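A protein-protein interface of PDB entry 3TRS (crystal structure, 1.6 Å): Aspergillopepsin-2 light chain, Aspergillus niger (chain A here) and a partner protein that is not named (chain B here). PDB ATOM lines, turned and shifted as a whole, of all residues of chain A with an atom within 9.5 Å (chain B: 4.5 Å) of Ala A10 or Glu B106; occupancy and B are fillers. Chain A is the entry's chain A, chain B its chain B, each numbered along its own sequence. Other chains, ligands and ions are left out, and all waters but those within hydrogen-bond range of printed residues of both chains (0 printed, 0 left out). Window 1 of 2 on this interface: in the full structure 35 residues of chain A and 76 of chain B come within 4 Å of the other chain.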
ATOM      1  N   GLU A   2      18.018  -9.739 -18.918  1.00  0.00           N
ATOM      2  CA  GLU A   2      18.276 -11.207 -18.919  1.00  0.00           C
ATOM      3  C   GLU A   2      17.995 -11.763 -20.287  1.00  0.00           C
ATOM      4  O   GLU A   2      17.035 -11.366 -20.952  1.00  0.00           O
ATOM      5  CB  GLU A   2      17.365 -11.930 -17.934  1.00  0.00           C
ATOM      6  CG  GLU A   2      17.857 -11.998 -16.499  1.00  0.00           C
ATOM      7  CD  GLU A   2      17.155 -13.097 -15.709  1.00  0.00           C
ATOM      8  OE1 GLU A   2      16.628 -14.050 -16.338  1.00  0.00           O
ATOM      9  OE2 GLU A   2      17.131 -13.010 -14.458  1.00  0.00           O
ATOM     10  N   TRP A   7      12.254 -17.267 -23.587  1.00  0.00           N
ATOM     11  CA  TRP A   7      11.317 -16.307 -23.021  1.00  0.00           C
ATOM     12  C   TRP A   7      11.745 -14.918 -23.276  1.00  0.00           C
ATOM     13  O   TRP A   7      12.880 -14.542 -22.993  1.00  0.00           O
ATOM     14  CB  TRP A   7      11.239 -16.428 -21.529  1.00  0.00           C
ATOM     15  CG  TRP A   7      10.454 -17.542 -21.041  1.00  0.00           C
ATOM     16  CD1 TRP A   7      10.132 -18.692 -21.706  1.00  0.00           C
ATOM     17  CD2 TRP A   7       9.934 -17.659 -19.739  1.00  0.00           C
ATOM     18  NE1 TRP A   7       9.422 -19.524 -20.875  1.00  0.00           N
ATOM     19  CE2 TRP A   7       9.278 -18.901 -19.664  1.00  0.00           C
ATOM     20  CE3 TRP A   7       9.958 -16.830 -18.612  1.00  0.00           C
ATOM     21  CZ2 TRP A   7       8.659 -19.336 -18.505  1.00  0.00           C
ATOM     22  CZ3 TRP A   7       9.335 -17.252 -17.476  1.00  0.00           C
ATOM     23  CH2 TRP A   7       8.683 -18.492 -17.427  1.00  0.00           C
ATOM     24  N   ALA A   8      10.802 -14.124 -23.731  1.00  0.00           N
ATOM     25  CA  ALA A   8      11.013 -12.712 -23.793  1.00  0.00           C
ATOM     26  C   ALA A   8       9.869 -12.154 -22.994  1.00  0.00           C
ATOM     27  O   ALA A   8       8.798 -12.765 -22.920  1.00  0.00           O
ATOM     28  CB  ALA A   8      10.967 -12.228 -25.208  1.00  0.00           C
ATOM     29  N   GLY A   9      10.103 -11.021 -22.369  1.00  0.00           N
ATOM     30  CA  GLY A   9       9.036 -10.366 -21.668  1.00  0.00           C
ATOM     31  C   GLY A   9       9.477  -9.987 -20.303  1.00  0.00           C
ATOM     32  O   GLY A   9      10.634  -9.632 -20.074  1.00  0.00           O
ATOM     33  N   ALA A  10       8.539 -10.048 -19.388  1.00  0.00           N
ATOM     34  CA  ALA A  10       8.738  -9.404 -18.123  1.00  0.00           C
ATOM     35  C   ALA A  10       8.348 -10.398 -17.103  1.00  0.00           C
ATOM     36  O   ALA A  10       7.300 -10.983 -17.176  1.00  0.00           O
ATOM     37  CB  ALA A  10       7.894  -8.202 -18.017  1.00  0.00           C
ATOM     38  N   VAL A  11       9.215 -10.607 -16.142  1.00  0.00           N
ATOM     39  CA  VAL A  11       8.913 -11.559 -15.133  1.00  0.00           C
ATOM     40  C   VAL A  11       9.034 -10.797 -13.852  1.00  0.00           C
ATOM     41  O   VAL A  11      10.105 -10.255 -13.554  1.00  0.00           O
ATOM     42  CB  VAL A  11       9.905 -12.731 -15.116  1.00  0.00           C
ATOM     43  CG1 VAL A  11       9.625 -13.629 -13.935  1.00  0.00           C
ATOM     44  CG2 VAL A  11       9.840 -13.518 -16.419  1.00  0.00           C
ATOM     45  N   LEU A  12       7.936 -10.730 -13.118  1.00  0.00           N
ATOM     46  CA  LEU A  12       7.989 -10.260 -11.758  1.00  0.00           C
ATOM     47  C   LEU A  12       8.415 -11.396 -10.885  1.00  0.00           C
ATOM     48  O   LEU A  12       7.944 -12.525 -11.016  1.00  0.00           O
ATOM     49  CB  LEU A  12       6.644  -9.762 -11.305  1.00  0.00           C
ATOM     50  CG  LEU A  12       6.255  -8.431 -11.916  1.00  0.00           C
ATOM     51  CD1 LEU A  12       4.807  -8.264 -11.572  1.00  0.00           C
ATOM     52  CD2 LEU A  12       7.095  -7.279 -11.367  1.00  0.00           C
ATOM     53  N   ILE A  13       9.344 -11.097 -10.002  1.00  0.00           N
ATOM     54  CA  ILE A  13       9.770 -12.065  -9.055  1.00  0.00           C
ATOM     55  C   ILE A  13       9.381 -11.463  -7.741  1.00  0.00           C
ATOM     56  O   ILE A  13       9.749 -10.346  -7.417  1.00  0.00           O
ATOM     57  CB  ILE A  13      11.276 -12.325  -9.142  1.00  0.00           C
ATOM     58  CG1 ILE A  13      11.603 -12.908 -10.528  1.00  0.00           C
ATOM     59  CG2 ILE A  13      11.695 -13.287  -8.019  1.00  0.00           C
ATOM     60  CD1 ILE A  13      13.077 -12.900 -10.885  1.00  0.00           C
ATOM     61  N   GLY A  14       8.592 -12.209  -7.012  1.00  0.00           N
ATOM     62  CA  GLY A  14       8.121 -11.756  -5.733  1.00  0.00           C
ATOM     63  C   GLY A  14       7.405 -12.899  -5.108  1.00  0.00           C
ATOM     64  O   GLY A  14       7.872 -14.028  -5.153  1.00  0.00           O
ATOM     65  N   TYR A  17       1.938 -14.065  -6.045  1.00  0.00           N
ATOM     66  CA  TYR A  17       1.234 -13.765  -7.292  1.00  0.00           C
ATOM     67  C   TYR A  17       0.122 -14.768  -7.480  1.00  0.00           C
ATOM     68  O   TYR A  17       0.340 -15.961  -7.578  1.00  0.00           O
ATOM     69  CB  TYR A  17       2.138 -13.802  -8.484  1.00  0.00           C
ATOM     70  CG  TYR A  17       3.168 -12.744  -8.394  1.00  0.00           C
ATOM     71  CD1 TYR A  17       2.814 -11.403  -8.331  1.00  0.00           C
ATOM     72  CD2 TYR A  17       4.493 -13.090  -8.329  1.00  0.00           C
ATOM     73  CE1 TYR A  17       3.793 -10.431  -8.233  1.00  0.00           C
ATOM     74  CE2 TYR A  17       5.462 -12.152  -8.245  1.00  0.00           C
ATOM     75  CZ  TYR A  17       5.120 -10.835  -8.188  1.00  0.00           C
ATOM     76  OH  TYR A  17       6.137  -9.929  -8.099  1.00  0.00           O
ATOM     77  N   THR A  18      -1.084 -14.262  -7.549  1.00  0.00           N
ATOM     78  CA  THR A  18      -2.212 -15.128  -7.685  1.00  0.00           C
ATOM     79  C   THR A  18      -2.973 -14.752  -8.920  1.00  0.00           C
ATOM     80  O   THR A  18      -3.952 -15.364  -9.252  1.00  0.00           O
ATOM     81  CB  THR A  18      -3.138 -14.990  -6.493  1.00  0.00           C
ATOM     82  OG1 THR A  18      -3.456 -13.605  -6.339  1.00  0.00           O
ATOM     83  CG2 THR A  18      -2.454 -15.535  -5.264  1.00  0.00           C
ATOM     84  N   LYS A  19      -2.539 -13.705  -9.579  1.00  0.00           N
ATOM     85  CA  LYS A  19      -3.266 -13.274 -10.752  1.00  0.00           C
ATOM     86  C   LYS A  19      -2.333 -12.533 -11.641  1.00  0.00           C
ATOM     87  O   LYS A  19      -1.580 -11.670 -11.208  1.00  0.00           O
ATOM     88  CB  LYS A  19      -4.450 -12.384 -10.372  1.00  0.00           C
ATOM     89  CG  LYS A  19      -5.381 -12.109 -11.520  1.00  0.00           C
ATOM     90  CD  LYS A  19      -6.549 -11.256 -11.056  1.00  0.00           C
ATOM     91  CE  LYS A  19      -7.497 -10.932 -12.207  1.00  0.00           C
ATOM     92  NZ  LYS A  19      -7.280  -9.546 -12.742  1.00  0.00           N
ATOM     93  N   VAL A  20      -2.345 -12.897 -12.909  1.00  0.00           N
ATOM     94  CA  VAL A  20      -1.578 -12.144 -13.860  1.00  0.00           C
ATOM     95  C   VAL A  20      -2.471 -11.999 -15.036  1.00  0.00           C
ATOM     96  O   VAL A  20      -3.172 -12.914 -15.420  1.00  0.00           O
ATOM     97  CB  VAL A  20      -0.310 -12.841 -14.340  1.00  0.00           C
ATOM     98  CG1 VAL A  20       0.516 -11.847 -15.189  1.00  0.00           C
ATOM     99  CG2 VAL A  20       0.491 -13.355 -13.167  1.00  0.00           C
ATOM    100  N   THR A  21      -2.433 -10.821 -15.588  1.00  0.00           N
ATOM    101  CA  THR A  21      -3.280 -10.538 -16.688  1.00  0.00           C
ATOM    102  C   THR A  21      -2.571  -9.574 -17.579  1.00  0.00           C
ATOM    103  O   THR A  21      -1.659  -8.850 -17.175  1.00  0.00           O
ATOM    104  CB  THR A  21      -4.622  -9.989 -16.213  1.00  0.00           C
ATOM    105  OG1 THR A  21      -5.481  -9.853 -17.347  1.00  0.00           O
ATOM    106  CG2 THR A  21      -4.440  -8.655 -15.504  1.00  0.00           C
ATOM    107  N   GLY A  22      -2.959  -9.622 -18.836  1.00  0.00           N
ATOM    108  CA  GLY A  22      -2.374  -8.761 -19.803  1.00  0.00           C
ATOM    109  C   GLY A  22      -3.327  -8.831 -20.940  1.00  0.00           C
ATOM    110  O   GLY A  22      -4.150  -9.737 -21.044  1.00  0.00           O
ATOM    111  N   GLU A  23      -3.265  -7.813 -21.744  1.00  0.00           N
ATOM    112  CA  GLU A  23      -4.119  -7.751 -22.876  1.00  0.00           C
ATOM    113  C   GLU A  23      -3.233  -7.411 -24.014  1.00  0.00           C
ATOM    114  O   GLU A  23      -2.336  -6.589 -23.896  1.00  0.00           O
ATOM    115  CB  GLU A  23      -5.167  -6.686 -22.682  1.00  0.00           C
ATOM    116  CG  GLU A  23      -5.946  -6.395 -23.936  1.00  0.00           C
ATOM    117  CD  GLU A  23      -6.886  -5.226 -23.748  1.00  0.00           C
ATOM    118  OE1 GLU A  23      -7.246  -4.947 -22.587  1.00  0.00           O
ATOM    119  OE2 GLU A  23      -7.245  -4.580 -24.753  1.00  0.00           O
ATOM    120  N   PHE A  24      -3.433  -8.070 -25.131  1.00  0.00           N
ATOM    121  CA  PHE A  24      -2.622  -7.699 -26.244  1.00  0.00           C
ATOM    122  C   PHE A  24      -3.440  -7.769 -27.476  1.00  0.00           C
ATOM    123  O   PHE A  24      -4.456  -8.453 -27.530  1.00  0.00           O
ATOM    124  CB  PHE A  24      -1.373  -8.562 -26.355  1.00  0.00           C
ATOM    125  CG  PHE A  24      -1.650 -10.017 -26.376  1.00  0.00           C
ATOM    126  CD1 PHE A  24      -1.628 -10.753 -25.207  1.00  0.00           C
ATOM    127  CD2 PHE A  24      -1.889 -10.665 -27.581  1.00  0.00           C
ATOM    128  CE1 PHE A  24      -1.890 -12.109 -25.208  1.00  0.00           C
ATOM    129  CE2 PHE A  24      -2.156 -12.030 -27.599  1.00  0.00           C
ATOM    130  CZ  PHE A  24      -2.136 -12.754 -26.422  1.00  0.00           C
ATOM    131  N   TRP B  10       2.043 -15.097 -23.577  1.00  0.00           N
ATOM    132  CA  TRP B  10       1.248 -15.620 -22.547  1.00  0.00           C
ATOM    133  C   TRP B  10       1.532 -14.873 -21.286  1.00  0.00           C
ATOM    134  O   TRP B  10       2.525 -14.156 -21.160  1.00  0.00           O
ATOM    135  CB  TRP B  10       1.478 -17.116 -22.375  1.00  0.00           C
ATOM    136  CG  TRP B  10       2.891 -17.553 -22.228  1.00  0.00           C
ATOM    137  CD1 TRP B  10       3.731 -17.939 -23.225  1.00  0.00           C
ATOM    138  CD2 TRP B  10       3.619 -17.707 -21.012  1.00  0.00           C
ATOM    139  NE1 TRP B  10       4.929 -18.336 -22.709  1.00  0.00           N
ATOM    140  CE2 TRP B  10       4.894 -18.190 -21.347  1.00  0.00           C
ATOM    141  CE3 TRP B  10       3.316 -17.494 -19.677  1.00  0.00           C
ATOM    142  CZ2 TRP B  10       5.864 -18.459 -20.392  1.00  0.00           C
ATOM    143  CZ3 TRP B  10       4.285 -17.769 -18.714  1.00  0.00           C
ATOM    144  CH2 TRP B  10       5.547 -18.225 -19.078  1.00  0.00           C
ATOM    145  N   VAL B  11       0.633 -15.059 -20.355  1.00  0.00           N
ATOM    146  CA  VAL B  11       0.853 -14.598 -19.019  1.00  0.00           C
ATOM    147  C   VAL B  11       0.870 -15.806 -18.155  1.00  0.00           C
ATOM    148  O   VAL B  11       0.250 -16.815 -18.454  1.00  0.00           O
ATOM    149  CB  VAL B  11      -0.252 -13.666 -18.557  1.00  0.00           C
ATOM    150  CG1 VAL B  11      -0.206 -12.409 -19.403  1.00  0.00           C
ATOM    151  CG2 VAL B  11      -1.580 -14.400 -18.673  1.00  0.00           C
ATOM    152  N   GLY B  12       1.572 -15.702 -17.056  1.00  0.00           N
ATOM    153  CA  GLY B  12       1.794 -16.867 -16.293  1.00  0.00           C
ATOM    154  C   GLY B  12       2.209 -16.484 -14.915  1.00  0.00           C
ATOM    155  O   GLY B  12       2.708 -15.386 -14.671  1.00  0.00           O
ATOM    156  N   ILE B  13       2.013 -17.448 -14.050  1.00  0.00           N
ATOM    157  CA  ILE B  13       2.523 -17.416 -12.717  1.00  0.00           C
ATOM    158  C   ILE B  13       3.559 -18.522 -12.685  1.00  0.00           C
ATOM    159  O   ILE B  13       3.286 -19.665 -13.070  1.00  0.00           O
ATOM    160  CB  ILE B  13       1.424 -17.669 -11.699  1.00  0.00           C
ATOM    161  CG1 ILE B  13       0.467 -16.483 -11.667  1.00  0.00           C
ATOM    162  CG2 ILE B  13       2.033 -17.883 -10.321  1.00  0.00           C
ATOM    163  CD1 ILE B  13      -0.820 -16.788 -10.960  1.00  0.00           C
ATOM    164  N   ASP B  14       4.756 -18.142 -12.264  1.00  0.00           N
ATOM    165  CA  ASP B  14       5.844 -19.069 -12.031  1.00  0.00           C
ATOM    166  C   ASP B  14       6.488 -19.528 -13.295  1.00  0.00           C
ATOM    167  O   ASP B  14       6.110 -19.095 -14.361  1.00  0.00           O
ATOM    168  CB  ASP B  14       5.376 -20.202 -11.139  1.00  0.00           C
ATOM    169  CG  ASP B  14       5.029 -19.689  -9.763  1.00  0.00           C
ATOM    170  OD1 ASP B  14       5.626 -18.657  -9.388  1.00  0.00           O
ATOM    171  OD2 ASP B  14       4.196 -20.284  -9.093  1.00  0.00           O
ATOM    172  N   ILE B  22       3.899 -23.843 -13.807  1.00  0.00           N
ATOM    173  CA  ILE B  22       3.608 -22.553 -14.392  1.00  0.00           C
ATOM    174  C   ILE B  22       2.149 -22.620 -14.675  1.00  0.00           C
ATOM    175  O   ILE B  22       1.665 -23.574 -15.253  1.00  0.00           O
ATOM    176  CB  ILE B  22       4.308 -22.287 -15.729  1.00  0.00           C
ATOM    177  CG1 ILE B  22       5.815 -22.548 -15.643  1.00  0.00           C
ATOM    178  CG2 ILE B  22       4.016 -20.861 -16.181  1.00  0.00           C
ATOM    179  CD1 ILE B  22       6.511 -22.488 -17.001  1.00  0.00           C
ATOM    180  N   ASN B 104       6.519 -15.938  -9.373  1.00  0.00           N
ATOM    181  CA  ASN B 104       6.760 -15.260 -10.613  1.00  0.00           C
ATOM    182  C   ASN B 104       5.455 -14.929 -11.250  1.00  0.00           C
ATOM    183  O   ASN B 104       4.509 -15.708 -11.187  1.00  0.00           O
ATOM    184  CB  ASN B 104       7.529 -16.100 -11.613  1.00  0.00           C
ATOM    185  CG  ASN B 104       8.784 -16.697 -11.050  1.00  0.00           C
ATOM    186  OD1 ASN B 104       9.195 -17.761 -11.493  1.00  0.00           O
ATOM    187  ND2 ASN B 104       9.418 -16.013 -10.105  1.00  0.00           N
ATOM    188  N   ALA B 105       5.422 -13.743 -11.816  1.00  0.00           N
ATOM    189  CA  ALA B 105       4.299 -13.298 -12.584  1.00  0.00           C
ATOM    190  C   ALA B 105       4.937 -12.789 -13.830  1.00  0.00           C
ATOM    191  O   ALA B 105       5.902 -11.998 -13.791  1.00  0.00           O
ATOM    192  CB  ALA B 105       3.558 -12.206 -11.884  1.00  0.00           C
ATOM    193  N   GLU B 106       4.404 -13.198 -14.959  1.00  0.00           N
ATOM    194  CA  GLU B 106       5.114 -12.893 -16.146  1.00  0.00           C
ATOM    195  C   GLU B 106       4.212 -12.696 -17.311  1.00  0.00           C
ATOM    196  O   GLU B 106       3.114 -13.257 -17.364  1.00  0.00           O
ATOM    197  CB  GLU B 106       6.145 -13.981 -16.476  1.00  0.00           C
ATOM    198  CG  GLU B 106       5.565 -15.367 -16.720  1.00  0.00           C
ATOM    199  CD  GLU B 106       5.686 -16.256 -15.531  1.00  0.00           C
ATOM    200  OE1 GLU B 106       6.343 -15.857 -14.556  1.00  0.00           O
ATOM    201  OE2 GLU B 106       5.082 -17.335 -15.547  1.00  0.00           O
ATOM    202  N   TRP B 107       4.720 -11.886 -18.212  1.00  0.00           N
ATOM    203  CA  TRP B 107       4.112 -11.633 -19.490  1.00  0.00           C
ATOM    204  C   TRP B 107       5.199 -11.964 -20.449  1.00  0.00           C
ATOM    205  O   TRP B 107       6.290 -11.346 -20.455  1.00  0.00           O
ATOM    206  CB  TRP B 107       3.737 -10.170 -19.646  1.00  0.00           C
ATOM    207  CG  TRP B 107       2.846  -9.702 -18.594  1.00  0.00           C
ATOM    208  CD1 TRP B 107       1.500  -9.643 -18.661  1.00  0.00           C
ATOM    209  CD2 TRP B 107       3.208  -9.299 -17.286  1.00  0.00           C
ATOM    210  NE1 TRP B 107       0.988  -9.198 -17.476  1.00  0.00           N
ATOM    211  CE2 TRP B 107       2.021  -8.965 -16.614  1.00  0.00           C
ATOM    212  CE3 TRP B 107       4.434  -9.146 -16.622  1.00  0.00           C
ATOM    213  CZ2 TRP B 107       2.008  -8.484 -15.297  1.00  0.00           C
ATOM    214  CZ3 TRP B 107       4.425  -8.663 -15.313  1.00  0.00           C
ATOM    215  CH2 TRP B 107       3.218  -8.347 -14.664  1.00  0.00           C
ATOM    216  N   ILE B 108       4.929 -12.960 -21.257  1.00  0.00           N
ATOM    217  CA  ILE B 108       5.998 -13.610 -21.927  1.00  0.00           C
ATOM    218  C   ILE B 108       5.598 -13.811 -23.331  1.00  0.00           C
ATOM    219  O   ILE B 108       4.462 -14.176 -23.621  1.00  0.00           O
ATOM    220  CB  ILE B 108       6.308 -14.973 -21.287  1.00  0.00           C
ATOM    221  CG1 ILE B 108       6.957 -14.819 -19.907  1.00  0.00           C
ATOM    222  CG2 ILE B 108       7.233 -15.776 -22.178  1.00  0.00           C
ATOM    223  CD1 ILE B 108       8.124 -13.871 -19.876  1.00  0.00           C
ATOM    224  N   PRO B 143       4.479  -4.407 -14.632  1.00  0.00           N
ATOM    225  CA  PRO B 143       5.740  -5.010 -14.999  1.00  0.00           C
ATOM    226  C   PRO B 143       6.926  -4.076 -14.804  1.00  0.00           C
ATOM    227  O   PRO B 143       8.030  -4.457 -15.135  1.00  0.00           O
ATOM    228  CB  PRO B 143       5.586  -5.273 -16.500  1.00  0.00           C
ATOM    229  CG  PRO B 143       4.205  -4.901 -16.854  1.00  0.00           C
ATOM    230  CD  PRO B 143       3.690  -4.006 -15.805  1.00  0.00           C
ATOM    231  N   ALA B 146       9.737  -5.537 -13.199  1.00  0.00           N
ATOM    232  CA  ALA B 146       9.975  -6.888 -13.660  1.00  0.00           C
ATOM    233  C   ALA B 146      11.367  -7.082 -14.212  1.00  0.00           C
ATOM    234  O   ALA B 146      12.017  -6.149 -14.696  1.00  0.00           O
ATOM    235  CB  ALA B 146       8.930  -7.303 -14.705  1.00  0.00           C
ATOM    236  N   THR B 147      11.824  -8.321 -14.125  1.00  0.00           N
ATOM    237  CA  THR B 147      13.002  -8.718 -14.843  1.00  0.00           C
ATOM    238  C   THR B 147      12.604  -8.801 -16.284  1.00  0.00           C
ATOM    239  O   THR B 147      11.636  -9.477 -16.636  1.00  0.00           O
ATOM    240  CB  THR B 147      13.522 -10.048 -14.366  1.00  0.00           C
ATOM    241  OG1 THR B 147      14.041  -9.865 -13.056  1.00  0.00           O
ATOM    242  CG2 THR B 147      14.629 -10.557 -15.284  1.00  0.00           C
ATOM    243  N   VAL B 163       9.307  -2.507 -20.781  1.00  0.00           N
ATOM    244  CA  VAL B 163       8.184  -2.505 -19.891  1.00  0.00           C
ATOM    245  C   VAL B 163       7.877  -1.071 -19.593  1.00  0.00           C
ATOM    246  O   VAL B 163       8.689  -0.178 -19.839  1.00  0.00           O
ATOM    247  CB  VAL B 163       8.427  -3.305 -18.588  1.00  0.00           C
ATOM    248  CG1 VAL B 163       8.671  -4.766 -18.914  1.00  0.00           C
ATOM    249  CG2 VAL B 163       9.619  -2.746 -17.805  1.00  0.00           C
ATOM    250  N   VAL B 168       4.109  -4.457 -21.278  1.00  0.00           N
ATOM    251  CA  VAL B 168       5.290  -5.185 -21.599  1.00  0.00           C
ATOM    252  C   VAL B 168       5.203  -5.231 -23.082  1.00  0.00           C
ATOM    253  O   VAL B 168       4.200  -5.662 -23.654  1.00  0.00           O
ATOM    254  CB  VAL B 168       5.244  -6.627 -21.102  1.00  0.00           C
ATOM    255  CG1 VAL B 168       6.545  -7.343 -21.480  1.00  0.00           C
ATOM    256  CG2 VAL B 168       5.018  -6.688 -19.596  1.00  0.00           C
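Along chain A the printed residues that touch a printed residue of chain B span positions 2 to 22.
Of the 16 printed residues of chain B, 13 touch a printed residue of chain A.
Among the printed residues, no Asp or Glu carboxylate lies within 4 Å of a Lys or Arg side-chain nitrogen of the other chain.
Ala A10 touches eight residues of chain B.
Glu B106 touches three residues of chain A.
Of chain A, only Val A20 (3.4 Å) comes within 4 Å of Gly B12.
Trp B107 touches just these residues of chain A: Ala A8 (3.8 Å), Gly A9 (3.2 Å), Ala A10 (2.8 Å), Leu A12 (3.5 Å), Val A20 (3.5 Å) and Thr A21 (2.7 Å).
Printed residues of chain B within 4 Å of Gly A22: Val B11.
Printed residues of chain B within 4 Å of Ile A13: Asn B104 (3.8 Å) and Thr B147 (3.9 Å).
Of the printed residues of chain A, Asn B104 touches Val A11 (3.99 Å), Leu A12 (3.0 Å), Ile A13 (3.8 Å) and Tyr A17 (3.6 Å).
Pro B143 touches none of the printed residues of chain A.
Glu A23 touches none of the printed residues of chain B.
The nearest residue of chain A that does not touch Glu B106 is Trp A7 (4.2 Å).
The backbone NH (N) of Glu B106 sits at hydrogen-bond distance from the backbone carbonyl oxygen (O) of Gly B12 (2.8 Å).
The backbone NH of Asp B14 lies within hydrogen-bond range of the side-chain carboxylate of Glu B106, 3.4 Å away.
The backbone NH (N) of Ile B13 lies within hydrogen-bond range of the side-chain carboxylate (OE2) of Glu B106, 3.4 Å away.
The backbone NH (N) of Asp B14 is in hydrogen-bond range of the backbone carbonyl oxygen (O) of Asn B104 (2.7 Å).
N of Trp B10 is in hydrogen-bond range of O of Ile B108 (2.6 Å).
Among the printed residues, pairs that only touch across the chains: Leu A12 with Asn B104, Ala A10 with Glu B106, Ala A8 with Ile B108, Gly A9 with Trp B107, Ala A10 with Thr B147, Val A11 with Ala B105, Trp A7 with Trp B10, Val A20 with Gly B12, Val A11 with Ala B146, Val A20 with Ile B13, Leu A12 with Trp B107, Val A20 with Ala B105, Val A20 with Trp B107, Tyr A17 with Ala B105, Tyr A17 with Asn B104, Gly A9 with Thr B147, Ala A10 with Ala B146, Thr A18 with Ile B13, Glu A2 with Thr B147, Ala A10 with Val B168, Ala A10 with Val B163, Leu A12 with Ala B146, Tyr A17 with Ile B13, Val A20 with Glu B106, Trp A7 with Ile B108, Val A11 with Glu B106, Lys A19 with Ile B13, Ala A8 with Trp B107, Ala A10 with Ala B105, Ile A13 with Asn B104, Ile A13 with Thr B147, Val A11 with Ile B108, Ala A10 with Ile B108, Val A20 with Val B11, Gly A9 with Val B168, Gly A22 with Val B11 and Val A11 with Asn B104.
N of Ala A10 is in hydrogen-bond range of O of Trp B107 (2.8 Å).
The backbone NH of Leu A12 is in hydrogen-bond range of the backbone carbonyl oxygen of Ala B105, 2.5 Å away.
The backbone NH (N) of Thr B147 is in hydrogen-bond range of the backbone carbonyl oxygen (O) of Val A11 (2.6 Å).
The indole nitrogen (NE1) of Trp B107 sits at hydrogen-bond distance from the backbone carbonyl oxygen (O) of Thr A21.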
